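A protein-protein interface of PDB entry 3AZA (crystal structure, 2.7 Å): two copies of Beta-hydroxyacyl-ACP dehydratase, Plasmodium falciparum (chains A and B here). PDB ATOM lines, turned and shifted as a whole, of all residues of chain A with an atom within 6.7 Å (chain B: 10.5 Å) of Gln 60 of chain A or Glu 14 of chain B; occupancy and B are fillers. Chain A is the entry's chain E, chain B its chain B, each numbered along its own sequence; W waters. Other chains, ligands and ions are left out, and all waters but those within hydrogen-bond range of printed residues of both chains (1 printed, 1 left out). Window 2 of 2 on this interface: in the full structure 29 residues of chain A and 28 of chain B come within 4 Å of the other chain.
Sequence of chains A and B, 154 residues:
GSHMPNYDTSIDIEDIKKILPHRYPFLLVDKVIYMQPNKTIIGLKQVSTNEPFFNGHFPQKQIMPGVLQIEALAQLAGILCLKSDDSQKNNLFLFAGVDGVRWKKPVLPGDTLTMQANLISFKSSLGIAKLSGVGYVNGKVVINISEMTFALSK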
ATOM      1  N   ASN A  55     -31.032  19.538  -0.092  1.00  0.00           N
ATOM      2  CA  ASN A  55     -30.923  18.081  -0.252  1.00  0.00           C
ATOM      3  C   ASN A  55     -31.491  17.603  -1.585  1.00  0.00           C
ATOM      4  O   ASN A  55     -30.966  16.658  -2.190  1.00  0.00           O
ATOM      5  CB  ASN A  55     -31.599  17.335   0.903  1.00  0.00           C
ATOM      6  CG  ASN A  55     -30.650  17.059   2.068  1.00  0.00           C
ATOM      7  OD1 ASN A  55     -29.540  17.597   2.132  1.00  0.00           O
ATOM      8  ND2 ASN A  55     -31.089  16.211   2.996  1.00  0.00           N
ATOM      9  N   HIS A  57     -31.810  19.647  -4.287  1.00  0.00           N
ATOM     10  CA  HIS A  57     -31.323  20.495  -5.375  1.00  0.00           C
ATOM     11  C   HIS A  57     -29.881  20.997  -5.170  1.00  0.00           C
ATOM     12  O   HIS A  57     -29.680  22.162  -4.800  1.00  0.00           O
ATOM     13  CB  HIS A  57     -32.277  21.683  -5.553  1.00  0.00           C
ATOM     14  CG  HIS A  57     -32.210  22.328  -6.902  1.00  0.00           C
ATOM     15  ND1 HIS A  57     -31.285  23.298  -7.216  1.00  0.00           N
ATOM     16  CD2 HIS A  57     -32.969  22.158  -8.011  1.00  0.00           C
ATOM     17  CE1 HIS A  57     -31.470  23.694  -8.464  1.00  0.00           C
ATOM     18  NE2 HIS A  57     -32.486  23.017  -8.969  1.00  0.00           N
ATOM     19  N   PHE A  58     -28.873  20.149  -5.404  1.00  0.00           N
ATOM     20  CA  PHE A  58     -29.008  18.747  -5.801  1.00  0.00           C
ATOM     21  C   PHE A  58     -28.140  17.912  -4.862  1.00  0.00           C
ATOM     22  O   PHE A  58     -27.212  18.446  -4.241  1.00  0.00           O
ATOM     23  CB  PHE A  58     -28.498  18.526  -7.228  1.00  0.00           C
ATOM     24  CG  PHE A  58     -29.197  19.343  -8.279  1.00  0.00           C
ATOM     25  CD1 PHE A  58     -30.362  18.878  -8.880  1.00  0.00           C
ATOM     26  CD2 PHE A  58     -28.663  20.555  -8.701  1.00  0.00           C
ATOM     27  CE1 PHE A  58     -31.001  19.615  -9.868  1.00  0.00           C
ATOM     28  CE2 PHE A  58     -29.288  21.300  -9.687  1.00  0.00           C
ATOM     29  CZ  PHE A  58     -30.462  20.830 -10.274  1.00  0.00           C
ATOM     30  N   PRO A  59     -28.421  16.597  -4.753  1.00  0.00           N
ATOM     31  CA  PRO A  59     -27.574  15.717  -3.944  1.00  0.00           C
ATOM     32  C   PRO A  59     -26.082  15.882  -4.234  1.00  0.00           C
ATOM     33  O   PRO A  59     -25.286  16.014  -3.302  1.00  0.00           O
ATOM     34  CB  PRO A  59     -28.035  14.323  -4.363  1.00  0.00           C
ATOM     35  CG  PRO A  59     -29.465  14.495  -4.679  1.00  0.00           C
ATOM     36  CD  PRO A  59     -29.618  15.888  -5.246  1.00  0.00           C
ATOM     37  N   GLN A  60     -25.716  15.901  -5.512  1.00  0.00           N
ATOM     38  CA  GLN A  60     -24.308  15.940  -5.917  1.00  0.00           C
ATOM     39  C   GLN A  60     -23.730  17.351  -5.951  1.00  0.00           C
ATOM     40  O   GLN A  60     -22.509  17.519  -5.945  1.00  0.00           O
ATOM     41  CB  GLN A  60     -24.110  15.293  -7.294  1.00  0.00           C
ATOM     42  CG  GLN A  60     -24.897  13.998  -7.531  1.00  0.00           C
ATOM     43  CD  GLN A  60     -24.186  12.755  -7.027  1.00  0.00           C
ATOM     44  OE1 GLN A  60     -23.360  12.812  -6.096  1.00  0.00           O
ATOM     45  NE2 GLN A  60     -24.512  11.613  -7.635  1.00  0.00           N
ATOM     46  N   LYS A  61     -24.605  18.356  -5.984  1.00  0.00           N
ATOM     47  CA  LYS A  61     -24.188  19.746  -6.140  1.00  0.00           C
ATOM     48  C   LYS A  61     -25.296  20.695  -5.687  1.00  0.00           C
ATOM     49  O   LYS A  61     -26.367  20.735  -6.301  1.00  0.00           O
ATOM     50  CB  LYS A  61     -23.843  20.001  -7.604  1.00  0.00           C
ATOM     51  CG  LYS A  61     -22.758  21.020  -7.851  1.00  0.00           C
ATOM     52  CD  LYS A  61     -22.397  21.001  -9.326  1.00  0.00           C
ATOM     53  CE  LYS A  61     -21.229  21.905  -9.633  1.00  0.00           C
ATOM     54  NZ  LYS A  61     -20.845  21.773 -11.085  1.00  0.00           N
ATOM     55  N   GLN A  62     -25.027  21.454  -4.622  1.00  0.00           N
ATOM     56  CA  GLN A  62     -26.020  22.354  -4.025  1.00  0.00           C
ATOM     57  C   GLN A  62     -26.095  23.726  -4.706  1.00  0.00           C
ATOM     58  O   GLN A  62     -25.184  24.551  -4.584  1.00  0.00           O
ATOM     59  CB  GLN A  62     -25.778  22.511  -2.517  1.00  0.00           C
ATOM     60  CG  GLN A  62     -25.867  21.193  -1.739  1.00  0.00           C
ATOM     61  CD  GLN A  62     -26.146  21.389  -0.261  1.00  0.00           C
ATOM     62  OE1 GLN A  62     -25.561  22.259   0.393  1.00  0.00           O
ATOM     63  NE2 GLN A  62     -27.035  20.565   0.277  1.00  0.00           N
ATOM     64  N   ILE A  63     -27.191  23.947  -5.429  1.00  0.00           N
ATOM     65  CA  ILE A  63     -27.454  25.211  -6.126  1.00  0.00           C
ATOM     66  C   ILE A  63     -28.829  25.718  -5.727  1.00  0.00           C
ATOM     67  O   ILE A  63     -29.822  24.996  -5.856  1.00  0.00           O
ATOM     68  CB  ILE A  63     -27.414  25.038  -7.661  1.00  0.00           C
ATOM     69  CG1 ILE A  63     -25.989  24.711  -8.122  1.00  0.00           C
ATOM     70  CG2 ILE A  63     -27.949  26.295  -8.374  1.00  0.00           C
ATOM     71  CD1 ILE A  63     -25.930  23.838  -9.366  1.00  0.00           C
ATOM     72  N   LEU A 108     -24.964  30.047  -4.299  1.00  0.00           N
ATOM     73  CA  LEU A 108     -24.498  28.891  -3.544  1.00  0.00           C
ATOM     74  C   LEU A 108     -24.608  29.093  -2.028  1.00  0.00           C
ATOM     75  O   LEU A 108     -24.846  30.213  -1.572  1.00  0.00           O
ATOM     76  CB  LEU A 108     -23.054  28.551  -3.947  1.00  0.00           C
ATOM     77  CG  LEU A 108     -22.728  28.352  -5.436  1.00  0.00           C
ATOM     78  CD1 LEU A 108     -21.241  28.097  -5.598  1.00  0.00           C
ATOM     79  CD2 LEU A 108     -23.543  27.228  -6.089  1.00  0.00           C
ATOM     80  N   PRO A 109     -24.478  28.000  -1.246  1.00  0.00           N
ATOM     81  CA  PRO A 109     -24.309  28.131   0.204  1.00  0.00           C
ATOM     82  C   PRO A 109     -23.065  28.961   0.529  1.00  0.00           C
ATOM     83  O   PRO A 109     -22.012  28.762  -0.076  1.00  0.00           O
ATOM     84  CB  PRO A 109     -24.125  26.680   0.669  1.00  0.00           C
ATOM     85  CG  PRO A 109     -24.860  25.868  -0.340  1.00  0.00           C
ATOM     86  CD  PRO A 109     -24.704  26.595  -1.651  1.00  0.00           C
ATOM     87  N   SER B  10      -8.899  28.703  -0.695  1.00  0.00           N
ATOM     88  CA  SER B  10     -10.363  28.925  -0.741  1.00  0.00           C
ATOM     89  C   SER B  10     -11.170  27.662  -1.082  1.00  0.00           C
ATOM     90  O   SER B  10     -10.618  26.712  -1.651  1.00  0.00           O
ATOM     91  CB  SER B  10     -10.712  30.066  -1.710  1.00  0.00           C
ATOM     92  OG  SER B  10     -10.421  29.724  -3.062  1.00  0.00           O
ATOM     93  N   ILE B  11     -12.469  27.658  -0.741  1.00  0.00           N
ATOM     94  CA  ILE B  11     -13.313  26.447  -0.878  1.00  0.00           C
ATOM     95  C   ILE B  11     -14.828  26.676  -1.120  1.00  0.00           C
ATOM     96  O   ILE B  11     -15.413  27.647  -0.627  1.00  0.00           O
ATOM     97  CB  ILE B  11     -13.037  25.443   0.303  1.00  0.00           C
ATOM     98  CG1 ILE B  11     -12.108  24.317  -0.174  1.00  0.00           C
ATOM     99  CG2 ILE B  11     -14.322  24.846   0.884  1.00  0.00           C
ATOM    100  CD1 ILE B  11     -11.083  23.868   0.865  1.00  0.00           C
ATOM    101  N   ASP B  12     -15.424  25.762  -1.902  1.00  0.00           N
ATOM    102  CA  ASP B  12     -16.884  25.603  -2.028  1.00  0.00           C
ATOM    103  C   ASP B  12     -17.363  24.342  -1.273  1.00  0.00           C
ATOM    104  O   ASP B  12     -16.580  23.407  -1.072  1.00  0.00           O
ATOM    105  CB  ASP B  12     -17.270  25.494  -3.511  1.00  0.00           C
ATOM    106  CG  ASP B  12     -16.564  24.333  -4.226  1.00  0.00           C
ATOM    107  OD1 ASP B  12     -15.327  24.186  -4.065  1.00  0.00           O
ATOM    108  OD2 ASP B  12     -17.246  23.566  -4.951  1.00  0.00           O
ATOM    109  N   ILE B  13     -18.649  24.302  -0.897  1.00  0.00           N
ATOM    110  CA  ILE B  13     -19.197  23.295   0.058  1.00  0.00           C
ATOM    111  C   ILE B  13     -19.311  21.819  -0.412  1.00  0.00           C
ATOM    112  O   ILE B  13     -19.582  20.923   0.395  1.00  0.00           O
ATOM    113  CB  ILE B  13     -20.560  23.771   0.675  1.00  0.00           C
ATOM    114  CG1 ILE B  13     -21.068  22.757   1.728  1.00  0.00           C
ATOM    115  CG2 ILE B  13     -21.603  23.988  -0.422  1.00  0.00           C
ATOM    116  CD1 ILE B  13     -21.939  23.371   2.806  1.00  0.00           C
ATOM    117  N   GLU B  14     -19.109  21.554  -1.697  1.00  0.00           N
ATOM    118  CA  GLU B  14     -19.145  20.172  -2.168  1.00  0.00           C
ATOM    119  C   GLU B  14     -17.958  19.402  -1.601  1.00  0.00           C
ATOM    120  O   GLU B  14     -18.066  18.211  -1.272  1.00  0.00           O
ATOM    121  CB  GLU B  14     -19.172  20.105  -3.697  1.00  0.00           C
ATOM    122  CG  GLU B  14     -20.350  20.852  -4.334  1.00  0.00           C
ATOM    123  CD  GLU B  14     -21.699  20.481  -3.716  1.00  0.00           C
ATOM    124  OE1 GLU B  14     -22.024  19.272  -3.630  1.00  0.00           O
ATOM    125  OE2 GLU B  14     -22.440  21.410  -3.323  1.00  0.00           O
ATOM    126  N   ASP B  15     -16.838  20.109  -1.458  1.00  0.00           N
ATOM    127  CA  ASP B  15     -15.623  19.540  -0.883  1.00  0.00           C
ATOM    128  C   ASP B  15     -15.703  19.409   0.637  1.00  0.00           C
ATOM    129  O   ASP B  15     -15.107  18.488   1.204  1.00  0.00           O
ATOM    130  CB  ASP B  15     -14.396  20.351  -1.310  1.00  0.00           C
ATOM    131  CG  ASP B  15     -14.151  20.271  -2.812  1.00  0.00           C
ATOM    132  OD1 ASP B  15     -13.965  19.140  -3.327  1.00  0.00           O
ATOM    133  OD2 ASP B  15     -14.152  21.331  -3.481  1.00  0.00           O
ATOM    134  N   ILE B  16     -16.444  20.310   1.285  1.00  0.00           N
ATOM    135  CA  ILE B  16     -16.660  20.249   2.743  1.00  0.00           C
ATOM    136  C   ILE B  16     -17.346  18.932   3.159  1.00  0.00           C
ATOM    137  O   ILE B  16     -17.025  18.345   4.204  1.00  0.00           O
ATOM    138  CB  ILE B  16     -17.469  21.476   3.270  1.00  0.00           C
ATOM    139  CG1 ILE B  16     -16.763  22.793   2.893  1.00  0.00           C
ATOM    140  CG2 ILE B  16     -17.668  21.384   4.794  1.00  0.00           C
ATOM    141  CD1 ILE B  16     -17.466  24.077   3.373  1.00  0.00           C
ATOM    142  N   LYS B  17     -18.274  18.474   2.323  1.00  0.00           N
ATOM    143  CA  LYS B  17     -18.988  17.221   2.546  1.00  0.00           C
ATOM    144  C   LYS B  17     -18.125  15.985   2.259  1.00  0.00           C
ATOM    145  O   LYS B  17     -18.491  14.867   2.635  1.00  0.00           O
ATOM    146  CB  LYS B  17     -20.264  17.179   1.699  1.00  0.00           C
ATOM    147  CG  LYS B  17     -21.342  18.180   2.138  1.00  0.00           C
ATOM    148  CD  LYS B  17     -22.407  18.376   1.061  1.00  0.00           C
ATOM    149  CE  LYS B  17     -23.493  17.313   1.134  1.00  0.00           C
ATOM    150  NZ  LYS B  17     -24.797  17.860   0.645  1.00  0.00           N
ATOM    151  N   LYS B  18     -16.991  16.187   1.589  1.00  0.00           N
ATOM    152  CA  LYS B  18     -16.033  15.106   1.350  1.00  0.00           C
ATOM    153  C   LYS B  18     -15.095  14.964   2.536  1.00  0.00           C
ATOM    154  O   LYS B  18     -14.515  13.896   2.767  1.00  0.00           O
ATOM    155  CB  LYS B  18     -15.226  15.363   0.080  1.00  0.00           C
ATOM    156  CG  LYS B  18     -15.990  15.029  -1.186  1.00  0.00           C
ATOM    157  CD  LYS B  18     -15.376  15.739  -2.371  1.00  0.00           C
ATOM    158  CE  LYS B  18     -16.243  15.552  -3.594  1.00  0.00           C
ATOM    159  NZ  LYS B  18     -15.391  15.545  -4.809  1.00  0.00           N
ATOM    160  N   ILE B  19     -14.955  16.059   3.276  1.00  0.00           N
ATOM    161  CA  ILE B  19     -14.160  16.085   4.493  1.00  0.00           C
ATOM    162  C   ILE B  19     -15.031  15.643   5.671  1.00  0.00           C
ATOM    163  O   ILE B  19     -14.806  14.572   6.236  1.00  0.00           O
ATOM    164  CB  ILE B  19     -13.538  17.491   4.720  1.00  0.00           C
ATOM    165  CG1 ILE B  19     -12.726  17.911   3.484  1.00  0.00           C
ATOM    166  CG2 ILE B  19     -12.661  17.510   5.977  1.00  0.00           C
ATOM    167  CD1 ILE B  19     -12.698  19.414   3.224  1.00  0.00           C
ATOM    168  N   LEU B  20     -16.037  16.450   6.018  1.00  0.00           N
ATOM    169  CA  LEU B  20     -16.911  16.166   7.170  1.00  0.00           C
ATOM    170  C   LEU B  20     -17.983  15.117   6.856  1.00  0.00           C
ATOM    171  O   LEU B  20     -18.376  14.968   5.700  1.00  0.00           O
ATOM    172  CB  LEU B  20     -17.576  17.449   7.660  1.00  0.00           C
ATOM    173  CG  LEU B  20     -16.697  18.561   8.234  1.00  0.00           C
ATOM    174  CD1 LEU B  20     -17.531  19.834   8.409  1.00  0.00           C
ATOM    175  CD2 LEU B  20     -16.043  18.150   9.552  1.00  0.00           C
ATOM    176  N   PRO B  21     -18.455  14.381   7.882  1.00  0.00           N
ATOM    177  CA  PRO B  21     -19.531  13.412   7.642  1.00  0.00           C
ATOM    178  C   PRO B  21     -20.934  13.957   7.951  1.00  0.00           C
ATOM    179  O   PRO B  21     -21.930  13.358   7.534  1.00  0.00           O
ATOM    180  CB  PRO B  21     -19.167  12.251   8.576  1.00  0.00           C
ATOM    181  CG  PRO B  21     -18.451  12.908   9.728  1.00  0.00           C
ATOM    182  CD  PRO B  21     -17.883  14.237   9.243  1.00  0.00           C
ATOM    183  N   HIS B  22     -20.993  15.079   8.671  1.00  0.00           N
ATOM    184  CA  HIS B  22     -22.240  15.791   8.981  1.00  0.00           C
ATOM    185  C   HIS B  22     -23.058  16.076   7.726  1.00  0.00           C
ATOM    186  O   HIS B  22     -22.495  16.390   6.675  1.00  0.00           O
ATOM    187  CB  HIS B  22     -21.933  17.130   9.654  1.00  0.00           C
ATOM    188  CG  HIS B  22     -21.079  17.024  10.880  1.00  0.00           C
ATOM    189  ND1 HIS B  22     -19.752  16.650  10.836  1.00  0.00           N
ATOM    190  CD2 HIS B  22     -21.355  17.284  12.182  1.00  0.00           C
ATOM    191  CE1 HIS B  22     -19.255  16.661  12.060  1.00  0.00           C
ATOM    192  NE2 HIS B  22     -20.205  17.050  12.896  1.00  0.00           N
ATOM    193  N   ARG B  23     -24.380  15.966   7.836  1.00  0.00           N
ATOM    194  CA  ARG B  23     -25.275  16.343   6.739  1.00  0.00           C
ATOM    195  C   ARG B  23     -26.446  17.165   7.277  1.00  0.00           C
ATOM    196  O   ARG B  23     -26.443  17.561   8.451  1.00  0.00           O
ATOM    197  CB  ARG B  23     -25.773  15.106   5.973  1.00  0.00           C
ATOM    198  CG  ARG B  23     -24.703  14.330   5.186  1.00  0.00           C
ATOM    199  CD  ARG B  23     -24.055  15.158   4.080  1.00  0.00           C
ATOM    200  NE  ARG B  23     -23.037  14.406   3.336  1.00  0.00           N
ATOM    201  CZ  ARG B  23     -21.768  14.241   3.723  1.00  0.00           C
ATOM    202  NH1 ARG B  23     -21.327  14.777   4.861  1.00  0.00           N
ATOM    203  NH2 ARG B  23     -20.928  13.543   2.969  1.00  0.00           N
ATOM    204  N   LEU B  27     -25.030  20.003   9.316  1.00  0.00           N
ATOM    205  CA  LEU B  27     -23.866  20.667   8.740  1.00  0.00           C
ATOM    206  C   LEU B  27     -24.069  22.176   8.940  1.00  0.00           C
ATOM    207  O   LEU B  27     -25.077  22.750   8.488  1.00  0.00           O
ATOM    208  CB  LEU B  27     -23.734  20.306   7.257  1.00  0.00           C
ATOM    209  CG  LEU B  27     -22.601  20.847   6.382  1.00  0.00           C
ATOM    210  CD1 LEU B  27     -21.238  20.279   6.768  1.00  0.00           C
ATOM    211  CD2 LEU B  27     -22.900  20.490   4.937  1.00  0.00           C
ATOM    212  N   VAL B  29     -21.318  24.592   8.542  1.00  0.00           N
ATOM    213  CA  VAL B  29     -20.286  25.379   7.872  1.00  0.00           C
ATOM    214  C   VAL B  29     -20.641  25.460   6.390  1.00  0.00           C
ATOM    215  O   VAL B  29     -20.791  24.427   5.720  1.00  0.00           O
ATOM    216  CB  VAL B  29     -18.867  24.771   8.057  1.00  0.00           C
ATOM    217  CG1 VAL B  29     -17.825  25.579   7.295  1.00  0.00           C
ATOM    218  CG2 VAL B  29     -18.503  24.700   9.531  1.00  0.00           C
ATOM    219  N   ASP B  30     -20.780  26.684   5.888  1.00  0.00           N
ATOM    220  CA  ASP B  30     -21.169  26.908   4.501  1.00  0.00           C
ATOM    221  C   ASP B  30     -19.967  27.071   3.583  1.00  0.00           C
ATOM    222  O   ASP B  30     -19.984  26.636   2.426  1.00  0.00           O
ATOM    223  CB  ASP B  30     -22.061  28.140   4.393  1.00  0.00           C
ATOM    224  CG  ASP B  30     -23.426  27.925   5.004  1.00  0.00           C
ATOM    225  OD1 ASP B  30     -23.997  26.828   4.815  1.00  0.00           O
ATOM    226  OD2 ASP B  30     -23.930  28.861   5.664  1.00  0.00           O
ATOM    227  N   LYS B  31     -18.922  27.702   4.103  1.00  0.00           N
ATOM    228  CA  LYS B  31     -17.765  28.033   3.289  1.00  0.00           C
ATOM    229  C   LYS B  31     -16.515  28.167   4.142  1.00  0.00           C
ATOM    230  O   LYS B  31     -16.556  28.747   5.228  1.00  0.00           O
ATOM    231  CB  LYS B  31     -18.037  29.338   2.546  1.00  0.00           C
ATOM    232  CG  LYS B  31     -17.028  29.685   1.475  1.00  0.00           C
ATOM    233  CD  LYS B  31     -17.491  30.892   0.678  1.00  0.00           C
ATOM    234  CE  LYS B  31     -18.412  30.471  -0.452  1.00  0.00           C
ATOM    235  NZ  LYS B  31     -18.243  31.358  -1.638  1.00  0.00           N
ATOM    236  N   VAL B  32     -15.413  27.607   3.652  1.00  0.00           N
ATOM    237  CA  VAL B  32     -14.094  27.816   4.252  1.00  0.00           C
ATOM    238  C   VAL B  32     -13.353  28.843   3.390  1.00  0.00           C
ATOM    239  O   VAL B  32     -13.107  28.604   2.207  1.00  0.00           O
ATOM    240  CB  VAL B  32     -13.287  26.490   4.346  1.00  0.00           C
ATOM    241  CG1 VAL B  32     -11.850  26.752   4.787  1.00  0.00           C
ATOM    242  CG2 VAL B  32     -13.978  25.500   5.297  1.00  0.00           C
ATOM    243  N   ILE B  79     -12.464  20.321  10.446  1.00  0.00           N
ATOM    244  CA  ILE B  79     -11.949  20.390   9.070  1.00  0.00           C
ATOM    245  C   ILE B  79     -10.434  20.577   9.082  1.00  0.00           C
ATOM    246  O   ILE B  79      -9.709  19.901   8.343  1.00  0.00           O
ATOM    247  CB  ILE B  79     -12.598  21.539   8.259  1.00  0.00           C
ATOM    248  CG1 ILE B  79     -14.063  21.219   7.950  1.00  0.00           C
ATOM    249  CG2 ILE B  79     -11.838  21.767   6.959  1.00  0.00           C
ATOM    250  CD1 ILE B  79     -14.867  22.403   7.448  1.00  0.00           C
HETATM  251  O   HOH W   1     -21.987  24.017  -5.131  1.00  0.00           O
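Water W1 lies within hydrogen-bond range of the side-chain carboxylate of Glu 14 of chain B (3.2 Å) and the backbone carbonyl oxygen of Gln 62 of chain A (3.3 Å).
The side-chain carboxylate (OE2) of Glu 14 of chain B is in hydrogen-bond range of the backbone NH (N) of Gln 62 of chain A (2.9 Å).
The side-chain carboxylate of Glu 14 of chain B sits close to the backbone carbonyl oxygen of Gln 60 of chain A, 2.9 Å away.
No position is printed for both chains.
The backbone carbonyl oxygen (O) of Lys 17 of chain B is in hydrogen-bond range of the guanidinium group (NH2) of Arg 23 of chain B (2.8 Å).
Pro 59 of chain A touches none of the printed residues of chain B.
Gln 60 of chain A touches just one residue of chain B: Glu 14 (2.9 Å).
Of the printed residues of chain B, Lys 61 of chain A touches Glu 14 (3.3 Å).
Gln 62 of chain A touches just these residues of chain B: Glu 14 and Lys 17.
Of the printed residues of chain B, Pro 109 of chain A touches Ile 13 (3.8 Å) and Asp 30 (3.9 Å).
Glu 14 of chain B touches just these residues of chain A: Gln 60, Lys 61 and Gln 62.
Of the printed residues of chain A, Lys 17 of chain B touches Gln 62.
The nearest residue of chain B that does not touch Gln 60 of chain A is Lys 17 of chain B (6.5 Å).
The nearest printed residue of chain A that does not touch Lys 17 of chain B is Pro 59 of chain A (4.4 Å).
CA of Lys 61 of chain A touches OE1 of Glu 14 of chain B, at 3.3 Å.
NZ of Lys 17 of chain B touches NE2 of Gln 62 of chain A, at 3.5 Å.
Ile 13 of chain B touches Pro 109 of chain A (CG2 to CG, 3.8 Å).
O of Asp 30 of chain B touches O of Pro 109 of chain A, 3.9 Å away.
Printed residues of chain B that touch a printed residue of chain A: Ile 13, Glu 14, Lys 17 and Asp 30.
Hydrophobic or aromatic side chains of chain B that line the printed part of chain A: Ile 13.
Along chain B the printed residues that touch a printed residue of chain A span positions 13 to 30.
Of the 10 printed residues of chain A, 4 touch a printed residue of chain B.
Hydrophobic or aromatic side chains of chain A within 4 Å of the printed part of chain B: Pro 109.
Among the printed residues, 6 pairs touch across the chains.
Among the printed residues, no Asp or Glu carboxylate lies within 4 Å of a Lys or Arg side-chain nitrogen of the other chain.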
